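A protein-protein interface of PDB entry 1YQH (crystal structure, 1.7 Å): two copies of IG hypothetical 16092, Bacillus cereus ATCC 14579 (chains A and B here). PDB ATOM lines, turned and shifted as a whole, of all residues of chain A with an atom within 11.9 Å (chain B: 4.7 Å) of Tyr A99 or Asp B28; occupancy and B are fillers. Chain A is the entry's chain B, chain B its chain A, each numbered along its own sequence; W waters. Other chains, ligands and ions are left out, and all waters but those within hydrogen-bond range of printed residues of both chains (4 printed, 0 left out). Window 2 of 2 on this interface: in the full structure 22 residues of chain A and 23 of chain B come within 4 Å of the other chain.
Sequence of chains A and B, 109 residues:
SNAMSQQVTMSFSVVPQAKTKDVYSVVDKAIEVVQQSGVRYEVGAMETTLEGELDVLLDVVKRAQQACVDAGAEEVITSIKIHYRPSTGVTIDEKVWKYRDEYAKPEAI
Printed residues of chain B that touch a printed residue of chain A: Tyr B24, Asp B28, Ile B31, Gln B35 and Val B43. Printed residues of chain A that touch a printed residue of chain B: Arg A85, Glu A94, Val A96, Tyr A99 and Arg A100. Hydrophobic or aromatic side chains of chain A that line the printed part of chain B: Val A96 and Tyr A99. Along chain A the printed residues that touch a printed residue of chain B span positions 85 to 100. Among the printed residues, 8 pairs touch across the chains. Among the printed residues, no Asp or Glu carboxylate lies within 4 Å of a Lys or Arg side-chain nitrogen of the other chain.
Val B43 touches Val A96. Tyr A99 touches Ile B31 (CD2 to CG2, 3.6 Å). Tyr A99 touches Gln B35 (CD2 to OE1, 3.9999 Å). Tyr A99 touches Val B43.
OH of Tyr B24 lies within hydrogen-bond range of OE2 of Glu A94, at 2.5 Å. OH of Tyr A99 is in hydrogen-bond range of OD1 of Asp B28. The backbone carbonyl oxygen (O) of Val B43 sits at hydrogen-bond distance from the guanidinium group (NE) of Arg A100. The guanidinium group (NH2) of Arg A85 is in hydrogen-bond range of the side-chain hydroxyl (OH) of Tyr B24 (3.0 Å).
Water W2 lies within hydrogen-bond range of OH of Tyr A99, O of Tyr B24 and NZ of Lys A98. Water W3 lies within hydrogen-bond range of the backbone carbonyl oxygen (O) of Tyr A99 and the side-chain amide oxygen (OE1) of Gln B35. Water W1 bridges O of Tyr A99 (2.8 Å) and N of Val B43 (2.9 Å). Water W4 bridges O of Lys A98 (2.9 Å) and OE1 of Gln B35 (2.9 Å).
The backbone NH of Glu A94 is in hydrogen-bond range of the side-chain hydroxyl of Thr A91. The side-chain carboxylate (OE2) of Glu A42 lies within salt-bridge range of the guanidinium group (NH1) of Arg A100, at 2.7 Å. The backbone carbonyl oxygen (O) of Glu A94 lies close to the indole nitrogen (NE1) of Trp A97 (3.5 Å). The guanidinium group (NH1) of Arg A85 lies within salt-bridge range of the side-chain carboxylate (OE2) of Glu A94. The guanidinium group (NH2) of Arg A100 lies within salt-bridge range of the side-chain carboxylate (OE1) of Glu A102, at 3.3 Å.
No position is printed for both chains.
Printed residues of chain B within 4 Å of Tyr A99: Asp B28, Ile B31, Gln B35 and Val B43. Printed residues of chain A within 4 Å of Asp B28: Tyr A99. Ser B25 touches none of the printed residues of chain A. Val B27 touches none of the printed residues of chain A. No residue of chain A comes within 4 Å of Lys B29. No residue of chain A comes within 4 Å of Ala B30. Ile B31 touches just one residue of chain A: Tyr A99 (3.6 Å). No residue of chain A comes within 4 Å of Glu B32. Printed residues of chain A within 4 Å of Tyr B24: Arg A85 and Glu A94. Of the printed residues of chain B, Arg A100 touches Val B43 (2.8 Å). Of the printed residues of chain B, Glu A94 touches Tyr B24. Of the printed residues of chain A, Gln B35 touches Tyr A99 (3.9999 Å). Trp A97 touches none of the printed residues of chain B. The nearest printed residue of chain B that does not touch Tyr A99 is Val B27 (4.2 Å). The nearest printed residue of chain A that does not touch Asp B28 is Lys A98 (4.5 Å). The nearest printed residue of chain B that does not touch Val A96 is Tyr B24 (7.3 Å).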
ATOM      1  N   ARG A  40     -10.931  -7.455   0.820  1.00  0.00           N
ATOM      2  CA  ARG A  40     -11.432  -8.574   0.030  1.00  0.00           C
ATOM      3  C   ARG A  40     -10.290  -9.541  -0.288  1.00  0.00           C
ATOM      4  O   ARG A  40      -9.179  -9.123  -0.675  1.00  0.00           O
ATOM      5  CB  ARG A  40     -12.043  -8.071  -1.275  1.00  0.00           C
ATOM      6  CG  ARG A  40     -12.508  -9.215  -2.179  1.00  0.00           C
ATOM      7  CD  ARG A  40     -13.257  -8.745  -3.421  1.00  0.00           C
ATOM      8  NE  ARG A  40     -13.470  -9.889  -4.320  1.00  0.00           N
ATOM      9  CZ  ARG A  40     -14.080  -9.851  -5.502  1.00  0.00           C
ATOM     10  NH1 ARG A  40     -14.602  -8.723  -5.963  1.00  0.00           N
ATOM     11  NH2 ARG A  40     -14.184 -10.970  -6.215  1.00  0.00           N
ATOM     12  N   GLU A  42      -9.301 -13.998  -1.448  1.00  0.00           N
ATOM     13  CA  GLU A  42      -9.674 -15.380  -1.706  1.00  0.00           C
ATOM     14  C   GLU A  42      -8.464 -16.269  -1.509  1.00  0.00           C
ATOM     15  O   GLU A  42      -7.404 -16.008  -2.093  1.00  0.00           O
ATOM     16  CB  GLU A  42     -10.217 -15.549  -3.130  1.00  0.00           C
ATOM     17  CG  GLU A  42     -10.790 -16.943  -3.358  1.00  0.00           C
ATOM     18  CD  GLU A  42     -11.285 -17.149  -4.771  1.00  0.00           C
ATOM     19  OE1 GLU A  42     -12.464 -17.542  -4.918  1.00  0.00           O
ATOM     20  OE2 GLU A  42     -10.501 -16.930  -5.719  1.00  0.00           O
ATOM     21  N   HIS A  83      -0.263  -6.593  -9.261  1.00  0.00           N
ATOM     22  CA  HIS A  83      -0.687  -6.005 -10.527  1.00  0.00           C
ATOM     23  C   HIS A  83      -1.013  -4.533 -10.261  1.00  0.00           C
ATOM     24  O   HIS A  83      -1.994  -4.197  -9.561  1.00  0.00           O
ATOM     25  CB  HIS A  83      -1.909  -6.733 -11.090  1.00  0.00           C
ATOM     26  CG  HIS A  83      -2.248  -6.362 -12.502  1.00  0.00           C
ATOM     27  ND1 HIS A  83      -3.047  -7.156 -13.300  1.00  0.00           N
ATOM     28  CD2 HIS A  83      -1.892  -5.300 -13.263  1.00  0.00           C
ATOM     29  CE1 HIS A  83      -3.177  -6.591 -14.488  1.00  0.00           C
ATOM     30  NE2 HIS A  83      -2.483  -5.468 -14.493  1.00  0.00           N
ATOM     31  N   ARG A  85      -1.722  -0.731 -11.863  1.00  0.00           N
ATOM     32  CA  ARG A  85      -2.228  -0.012 -13.041  1.00  0.00           C
ATOM     33  C   ARG A  85      -2.881   1.289 -12.566  1.00  0.00           C
ATOM     34  O   ARG A  85      -4.110   1.369 -12.426  1.00  0.00           O
ATOM     35  CB  ARG A  85      -3.234  -0.860 -13.826  1.00  0.00           C
ATOM     36  CG  ARG A  85      -3.667  -0.227 -15.158  1.00  0.00           C
ATOM     37  CD  ARG A  85      -4.970  -0.867 -15.627  1.00  0.00           C
ATOM     38  NE  ARG A  85      -4.779  -2.245 -16.068  1.00  0.00           N
ATOM     39  CZ  ARG A  85      -5.672  -3.216 -15.917  1.00  0.00           C
ATOM     40  NH1 ARG A  85      -6.835  -2.967 -15.321  1.00  0.00           N
ATOM     41  NH2 ARG A  85      -5.399  -4.433 -16.362  1.00  0.00           N
ATOM     42  N   THR A  91      -8.785  -4.747 -10.321  1.00  0.00           N
ATOM     43  CA  THR A  91      -9.662  -5.481  -9.429  1.00  0.00           C
ATOM     44  C   THR A  91      -9.649  -6.968  -9.759  1.00  0.00           C
ATOM     45  O   THR A  91      -9.274  -7.368 -10.857  1.00  0.00           O
ATOM     46  CB  THR A  91     -11.120  -4.957  -9.513  1.00  0.00           C
ATOM     47  OG1 THR A  91     -11.618  -5.155 -10.847  1.00  0.00           O
ATOM     48  CG2 THR A  91     -11.168  -3.474  -9.159  1.00  0.00           C
ATOM     49  N   ILE A  92     -10.054  -7.785  -8.790  1.00  0.00           N
ATOM     50  CA  ILE A  92     -10.182  -9.215  -8.994  1.00  0.00           C
ATOM     51  C   ILE A  92     -11.207  -9.515 -10.094  1.00  0.00           C
ATOM     52  O   ILE A  92     -10.954 -10.327 -10.994  1.00  0.00           O
ATOM     53  CB  ILE A  92     -10.581  -9.919  -7.677  1.00  0.00           C
ATOM     54  CG1 ILE A  92      -9.403  -9.872  -6.689  1.00  0.00           C
ATOM     55  CG2 ILE A  92     -11.030 -11.369  -7.962  1.00  0.00           C
ATOM     56  CD1 ILE A  92      -9.734 -10.279  -5.258  1.00  0.00           C
ATOM     57  N   ASP A  93     -12.357  -8.855 -10.030  1.00  0.00           N
ATOM     58  CA  ASP A  93     -13.452  -9.193 -10.949  1.00  0.00           C
ATOM     59  C   ASP A  93     -13.084  -8.907 -12.403  1.00  0.00           C
ATOM     60  O   ASP A  93     -13.489  -9.636 -13.296  1.00  0.00           O
ATOM     61  CB  ASP A  93     -14.737  -8.457 -10.560  1.00  0.00           C
ATOM     62  CG  ASP A  93     -15.331  -8.952  -9.240  1.00  0.00           C
ATOM     63  OD1 ASP A  93     -16.043  -8.171  -8.578  1.00  0.00           O
ATOM     64  OD2 ASP A  93     -15.111 -10.118  -8.858  1.00  0.00           O
ATOM     65  N   GLU A  94     -12.308  -7.856 -12.645  1.00  0.00           N
ATOM     66  CA  GLU A  94     -11.935  -7.547 -14.019  1.00  0.00           C
ATOM     67  C   GLU A  94     -11.075  -8.652 -14.638  1.00  0.00           C
ATOM     68  O   GLU A  94     -11.140  -8.910 -15.844  1.00  0.00           O
ATOM     69  CB  GLU A  94     -11.255  -6.184 -14.100  1.00  0.00           C
ATOM     70  CG  GLU A  94      -9.772  -6.230 -14.018  1.00  0.00           C
ATOM     71  CD  GLU A  94      -9.168  -4.936 -14.436  1.00  0.00           C
ATOM     72  OE1 GLU A  94      -9.168  -4.001 -13.611  1.00  0.00           O
ATOM     73  OE2 GLU A  94      -8.712  -4.853 -15.597  1.00  0.00           O
ATOM     74  N   LYS A  95     -10.289  -9.325 -13.801  1.00  0.00           N
ATOM     75  CA  LYS A  95      -9.384 -10.363 -14.288  1.00  0.00           C
ATOM     76  C   LYS A  95     -10.050 -11.731 -14.424  1.00  0.00           C
ATOM     77  O   LYS A  95      -9.655 -12.521 -15.287  1.00  0.00           O
ATOM     78  CB  LYS A  95      -8.136 -10.426 -13.411  1.00  0.00           C
ATOM     79  CG  LYS A  95      -7.470  -9.047 -13.270  1.00  0.00           C
ATOM     80  CD  LYS A  95      -6.012  -9.110 -12.911  1.00  0.00           C
ATOM     81  CE  LYS A  95      -5.142  -9.675 -14.026  1.00  0.00           C
ATOM     82  NZ  LYS A  95      -3.806  -9.991 -13.427  1.00  0.00           N
ATOM     83  N   VAL A  96     -11.078 -12.003 -13.614  1.00  0.00           N
ATOM     84  CA  VAL A  96     -11.669 -13.346 -13.584  1.00  0.00           C
ATOM     85  C   VAL A  96     -13.070 -13.519 -14.180  1.00  0.00           C
ATOM     86  O   VAL A  96     -13.504 -14.652 -14.355  1.00  0.00           O
ATOM     87  CB  VAL A  96     -11.672 -13.967 -12.153  1.00  0.00           C
ATOM     88  CG1 VAL A  96     -10.272 -13.940 -11.545  1.00  0.00           C
ATOM     89  CG2 VAL A  96     -12.673 -13.265 -11.269  1.00  0.00           C
ATOM     90  N   TRP A  97     -13.771 -12.420 -14.477  1.00  0.00           N
ATOM     91  CA  TRP A  97     -15.176 -12.507 -14.896  1.00  0.00           C
ATOM     92  C   TRP A  97     -15.421 -13.413 -16.106  1.00  0.00           C
ATOM     93  O   TRP A  97     -16.461 -14.065 -16.180  1.00  0.00           O
ATOM     94  CB  TRP A  97     -15.790 -11.116 -15.136  1.00  0.00           C
ATOM     95  CG  TRP A  97     -15.282 -10.415 -16.368  1.00  0.00           C
ATOM     96  CD1 TRP A  97     -14.196  -9.601 -16.447  1.00  0.00           C
ATOM     97  CD2 TRP A  97     -15.850 -10.458 -17.693  1.00  0.00           C
ATOM     98  NE1 TRP A  97     -14.038  -9.135 -17.735  1.00  0.00           N
ATOM     99  CE2 TRP A  97     -15.044  -9.644 -18.517  1.00  0.00           C
ATOM    100  CE3 TRP A  97     -16.964 -11.102 -18.260  1.00  0.00           C
ATOM    101  CZ2 TRP A  97     -15.305  -9.458 -19.885  1.00  0.00           C
ATOM    102  CZ3 TRP A  97     -17.229 -10.912 -19.621  1.00  0.00           C
ATOM    103  CH2 TRP A  97     -16.400 -10.090 -20.415  1.00  0.00           C
ATOM    104  N   LYS A  98     -14.478 -13.446 -17.044  1.00  0.00           N
ATOM    105  CA  LYS A  98     -14.614 -14.263 -18.256  1.00  0.00           C
ATOM    106  C   LYS A  98     -14.512 -15.762 -17.949  1.00  0.00           C
ATOM    107  O   LYS A  98     -14.929 -16.604 -18.755  1.00  0.00           O
ATOM    108  CB  LYS A  98     -13.522 -13.895 -19.284  1.00  0.00           C
ATOM    109  CG  LYS A  98     -13.610 -12.473 -19.840  1.00  0.00           C
ATOM    110  CD  LYS A  98     -12.776 -12.324 -21.100  1.00  0.00           C
ATOM    111  CE  LYS A  98     -11.484 -11.533 -20.930  1.00  0.00           C
ATOM    112  NZ  LYS A  98     -10.963 -11.364 -19.563  1.00  0.00           N
ATOM    113  N   TYR A  99     -13.974 -16.087 -16.773  1.00  0.00           N
ATOM    114  CA  TYR A  99     -13.394 -17.410 -16.544  1.00  0.00           C
ATOM    115  C   TYR A  99     -13.991 -18.221 -15.410  1.00  0.00           C
ATOM    116  O   TYR A  99     -13.514 -19.326 -15.118  1.00  0.00           O
ATOM    117  CB  TYR A  99     -11.899 -17.267 -16.298  1.00  0.00           C
ATOM    118  CG  TYR A  99     -11.170 -16.584 -17.412  1.00  0.00           C
ATOM    119  CD1 TYR A  99     -10.381 -15.462 -17.164  1.00  0.00           C
ATOM    120  CD2 TYR A  99     -11.270 -17.054 -18.726  1.00  0.00           C
ATOM    121  CE1 TYR A  99      -9.689 -14.838 -18.187  1.00  0.00           C
ATOM    122  CE2 TYR A  99     -10.590 -16.429 -19.752  1.00  0.00           C
ATOM    123  CZ  TYR A  99      -9.810 -15.330 -19.483  1.00  0.00           C
ATOM    124  OH  TYR A  99      -9.129 -14.715 -20.502  1.00  0.00           O
ATOM    125  N   ARG A 100     -15.019 -17.676 -14.773  1.00  0.00           N
ATOM    126  CA  ARG A 100     -15.717 -18.365 -13.702  1.00  0.00           C
ATOM    127  C   ARG A 100     -17.223 -18.346 -13.930  1.00  0.00           C
ATOM    128  O   ARG A 100     -17.782 -17.300 -14.256  1.00  0.00           O
ATOM    129  CB  ARG A 100     -15.398 -17.699 -12.373  1.00  0.00           C
ATOM    130  CG  ARG A 100     -13.977 -17.923 -11.905  1.00  0.00           C
ATOM    131  CD  ARG A 100     -13.852 -17.429 -10.486  1.00  0.00           C
ATOM    132  NE  ARG A 100     -12.506 -17.596  -9.962  1.00  0.00           N
ATOM    133  CZ  ARG A 100     -12.208 -17.611  -8.666  1.00  0.00           C
ATOM    134  NH1 ARG A 100     -10.948 -17.765  -8.285  1.00  0.00           N
ATOM    135  NH2 ARG A 100     -13.169 -17.479  -7.750  1.00  0.00           N
ATOM    136  N   ASP A 101     -17.849 -19.508 -13.721  1.00  0.00           N
ATOM    137  CA  ASP A 101     -19.293 -19.707 -13.898  1.00  0.00           C
ATOM    138  C   ASP A 101     -20.154 -18.765 -13.070  1.00  0.00           C
ATOM    139  O   ASP A 101     -21.240 -18.359 -13.501  1.00  0.00           O
ATOM    140  CB  ASP A 101     -19.671 -21.166 -13.598  1.00  0.00           C
ATOM    141  CG  ASP A 101     -19.221 -22.113 -14.694  1.00  0.00           C
ATOM    142  OD1 ASP A 101     -18.703 -21.616 -15.707  1.00  0.00           O
ATOM    143  OD2 ASP A 101     -19.384 -23.343 -14.551  1.00  0.00           O
ATOM    144  N   GLU A 102     -19.658 -18.417 -11.888  1.00  0.00           N
ATOM    145  CA  GLU A 102     -20.390 -17.556 -10.948  1.00  0.00           C
ATOM    146  C   GLU A 102     -20.674 -16.151 -11.526  1.00  0.00           C
ATOM    147  O   GLU A 102     -21.482 -15.410 -10.966  1.00  0.00           O
ATOM    148  CB  GLU A 102     -19.687 -17.475  -9.582  1.00  0.00           C
ATOM    149  CG  GLU A 102     -18.285 -16.884  -9.607  1.00  0.00           C
ATOM    150  CD  GLU A 102     -17.666 -16.733  -8.224  1.00  0.00           C
ATOM    151  OE1 GLU A 102     -16.452 -17.015  -8.090  1.00  0.00           O
ATOM    152  OE2 GLU A 102     -18.385 -16.330  -7.273  1.00  0.00           O
ATOM    153  N   TYR A 103     -20.039 -15.811 -12.653  1.00  0.00           N
ATOM    154  CA  TYR A 103     -20.211 -14.495 -13.304  1.00  0.00           C
ATOM    155  C   TYR A 103     -21.215 -14.454 -14.463  1.00  0.00           C
ATOM    156  O   TYR A 103     -21.200 -13.516 -15.273  1.00  0.00           O
ATOM    157  CB  TYR A 103     -18.860 -13.939 -13.778  1.00  0.00           C
ATOM    158  CG  TYR A 103     -17.931 -13.542 -12.655  1.00  0.00           C
ATOM    159  CD1 TYR A 103     -17.157 -14.496 -12.000  1.00  0.00           C
ATOM    160  CD2 TYR A 103     -17.813 -12.205 -12.257  1.00  0.00           C
ATOM    161  CE1 TYR A 103     -16.298 -14.138 -10.970  1.00  0.00           C
ATOM    162  CE2 TYR A 103     -16.956 -11.832 -11.229  1.00  0.00           C
ATOM    163  CZ  TYR A 103     -16.207 -12.803 -10.585  1.00  0.00           C
ATOM    164  OH  TYR A 103     -15.351 -12.447  -9.568  1.00  0.00           O
ATOM    165  N   ALA A 104     -22.088 -15.452 -14.541  1.00  0.00           N
ATOM    166  CA  ALA A 104     -23.099 -15.515 -15.606  1.00  0.00           C
ATOM    167  C   ALA A 104     -24.284 -14.576 -15.357  1.00  0.00           C
ATOM    168  O   ALA A 104     -24.210 -13.364 -15.588  1.00  0.00           O
ATOM    169  CB  ALA A 104     -23.592 -16.935 -15.771  1.00  0.00           C
ATOM    170  N   TYR B  24      -5.255  -9.045 -22.695  1.00  0.00           N
ATOM    171  CA  TYR B  24      -6.366  -9.950 -22.362  1.00  0.00           C
ATOM    172  C   TYR B  24      -6.735 -10.880 -23.520  1.00  0.00           C
ATOM    173  O   TYR B  24      -7.149 -12.017 -23.286  1.00  0.00           O
ATOM    174  CB  TYR B  24      -7.622  -9.198 -21.895  1.00  0.00           C
ATOM    175  CG  TYR B  24      -7.538  -8.527 -20.528  1.00  0.00           C
ATOM    176  CD1 TYR B  24      -8.375  -7.452 -20.220  1.00  0.00           C
ATOM    177  CD2 TYR B  24      -6.632  -8.954 -19.550  1.00  0.00           C
ATOM    178  CE1 TYR B  24      -8.321  -6.814 -18.972  1.00  0.00           C
ATOM    179  CE2 TYR B  24      -6.567  -8.312 -18.289  1.00  0.00           C
ATOM    180  CZ  TYR B  24      -7.420  -7.250 -18.017  1.00  0.00           C
ATOM    181  OH  TYR B  24      -7.369  -6.616 -16.791  1.00  0.00           O
ATOM    182  N   SER B  25      -6.599 -10.398 -24.758  1.00  0.00           N
ATOM    183  CA  SER B  25      -6.898 -11.215 -25.939  1.00  0.00           C
ATOM    184  C   SER B  25      -5.943 -12.407 -26.053  1.00  0.00           C
ATOM    185  O   SER B  25      -6.342 -13.513 -26.422  1.00  0.00           O
ATOM    186  CB  SER B  25      -6.860 -10.364 -27.214  1.00  0.00           C
ATOM    187  OG  SER B  25      -7.762  -9.270 -27.105  1.00  0.00           O
ATOM    188  N   VAL B  26      -4.680 -12.154 -25.732  1.00  0.00           N
ATOM    189  CA  VAL B  26      -3.624 -13.152 -25.813  1.00  0.00           C
ATOM    190  C   VAL B  26      -3.787 -14.132 -24.651  1.00  0.00           C
ATOM    191  O   VAL B  26      -3.759 -15.349 -24.848  1.00  0.00           O
ATOM    192  CB  VAL B  26      -2.250 -12.461 -25.762  1.00  0.00           C
ATOM    193  CG1 VAL B  26      -1.131 -13.491 -25.719  1.00  0.00           C
ATOM    194  CG2 VAL B  26      -2.099 -11.531 -26.972  1.00  0.00           C
ATOM    195  N   VAL B  27      -3.995 -13.597 -23.451  1.00  0.00           N
ATOM    196  CA  VAL B  27      -4.195 -14.445 -22.273  1.00  0.00           C
ATOM    197  C   VAL B  27      -5.417 -15.382 -22.433  1.00  0.00           C
ATOM    198  O   VAL B  27      -5.390 -16.525 -21.970  1.00  0.00           O
ATOM    199  CB  VAL B  27      -4.239 -13.625 -20.944  1.00  0.00           C
ATOM    200  CG1 VAL B  27      -4.557 -14.539 -19.748  1.00  0.00           C
ATOM    201  CG2 VAL B  27      -2.899 -12.901 -20.714  1.00  0.00           C
ATOM    202  N   ASP B  28      -6.462 -14.907 -23.103  1.00  0.00           N
ATOM    203  CA  ASP B  28      -7.653 -15.722 -23.303  1.00  0.00           C
ATOM    204  C   ASP B  28      -7.372 -17.019 -24.082  1.00  0.00           C
ATOM    205  O   ASP B  28      -8.061 -18.023 -23.896  1.00  0.00           O
ATOM    206  CB  ASP B  28      -8.725 -14.898 -24.004  1.00  0.00           C
ATOM    207  CG  ASP B  28     -10.055 -15.587 -24.024  1.00  0.00           C
ATOM    208  OD1 ASP B  28     -10.638 -15.805 -22.940  1.00  0.00           O
ATOM    209  OD2 ASP B  28     -10.521 -15.900 -25.128  1.00  0.00           O
ATOM    210  N   LYS B  29      -6.356 -16.999 -24.942  1.00  0.00           N
ATOM    211  CA  LYS B  29      -5.967 -18.188 -25.691  1.00  0.00           C
ATOM    212  C   LYS B  29      -5.181 -19.159 -24.808  1.00  0.00           C
ATOM    213  O   LYS B  29      -5.277 -20.382 -24.974  1.00  0.00           O
ATOM    214  CB  LYS B  29      -5.170 -17.804 -26.941  1.00  0.00           C
ATOM    215  CG  LYS B  29      -5.959 -16.940 -27.949  1.00  0.00           C
ATOM    216  CD  LYS B  29      -7.286 -17.566 -28.383  1.00  0.00           C
ATOM    217  CE  LYS B  29      -7.105 -18.730 -29.329  1.00  0.00           C
ATOM    218  NZ  LYS B  29      -8.427 -19.240 -29.845  1.00  0.00           N
ATOM    219  N   ALA B  30      -4.414 -18.617 -23.867  1.00  0.00           N
ATOM    220  CA  ALA B  30      -3.721 -19.453 -22.887  1.00  0.00           C
ATOM    221  C   ALA B  30      -4.736 -20.132 -21.966  1.00  0.00           C
ATOM    222  O   ALA B  30      -4.647 -21.333 -21.721  1.00  0.00           O
ATOM    223  CB  ALA B  30      -2.713 -18.630 -22.077  1.00  0.00           C
ATOM    224  N   ILE B  31      -5.719 -19.378 -21.475  1.00  0.00           N
ATOM    225  CA  ILE B  31      -6.735 -19.986 -20.600  1.00  0.00           C
ATOM    226  C   ILE B  31      -7.570 -21.024 -21.367  1.00  0.00           C
ATOM    227  O   ILE B  31      -7.969 -22.049 -20.802  1.00  0.00           O
ATOM    228  CB  ILE B  31      -7.601 -18.906 -19.906  1.00  0.00           C
ATOM    229  CG1 ILE B  31      -6.723 -17.990 -19.033  1.00  0.00           C
ATOM    230  CG2 ILE B  31      -8.727 -19.555 -19.080  1.00  0.00           C
ATOM    231  CD1 ILE B  31      -5.979 -18.702 -17.933  1.00  0.00           C
ATOM    232  N   GLU B  32      -7.797 -20.788 -22.660  1.00  0.00           N
ATOM    233  CA  GLU B  32      -8.507 -21.765 -23.499  1.00  0.00           C
ATOM    234  C   GLU B  32      -7.804 -23.129 -23.468  1.00  0.00           C
ATOM    235  O   GLU B  32      -8.459 -24.183 -23.401  1.00  0.00           O
ATOM    236  CB  GLU B  32      -8.629 -21.251 -24.931  1.00  0.00           C
ATOM    237  CG  GLU B  32      -9.487 -22.119 -25.835  1.00  0.00           C
ATOM    238  CD  GLU B  32      -9.644 -21.519 -27.218  1.00  0.00           C
ATOM    239  OE1 GLU B  32     -10.798 -21.250 -27.615  1.00  0.00           O
ATOM    240  OE2 GLU B  32      -8.616 -21.308 -27.896  1.00  0.00           O
ATOM    241  N   GLN B  35      -8.812 -24.679 -20.345  1.00  0.00           N
ATOM    242  CA  GLN B  35     -10.235 -25.049 -20.386  1.00  0.00           C
ATOM    243  C   GLN B  35     -10.445 -26.331 -21.178  1.00  0.00           C
ATOM    244  O   GLN B  35     -11.314 -27.146 -20.839  1.00  0.00           O
ATOM    245  CB  GLN B  35     -11.061 -23.909 -20.976  1.00  0.00           C
ATOM    246  CG  GLN B  35     -11.158 -22.680 -20.029  1.00  0.00           C
ATOM    247  CD  GLN B  35     -11.785 -21.455 -20.680  1.00  0.00           C
ATOM    248  OE1 GLN B  35     -12.457 -20.650 -20.014  1.00  0.00           O
ATOM    249  NE2 GLN B  35     -11.579 -21.309 -21.973  1.00  0.00           N
ATOM    250  N   VAL B  43      -9.365 -20.413 -12.332  1.00  0.00           N
ATOM    251  CA  VAL B  43      -8.721 -19.175 -12.735  1.00  0.00           C
ATOM    252  C   VAL B  43      -8.827 -18.149 -11.594  1.00  0.00           C
ATOM    253  O   VAL B  43      -9.925 -17.850 -11.101  1.00  0.00           O
ATOM    254  CB  VAL B  43      -9.335 -18.622 -14.046  1.00  0.00           C
ATOM    255  CG1 VAL B  43      -8.650 -17.310 -14.437  1.00  0.00           C
ATOM    256  CG2 VAL B  43      -9.189 -19.654 -15.190  1.00  0.00           C
HETATM  257  O   HOH W   1     -12.090 -20.771 -13.195  1.00  0.00           O
HETATM  258  O   HOH W   2      -8.090 -12.427 -20.469  1.00  0.00           O
HETATM  259  O   HOH W   3     -13.152 -20.933 -17.259  1.00  0.00           O
HETATM  260  O   HOH W   4     -13.910 -18.247 -20.890  1.00  0.00           O
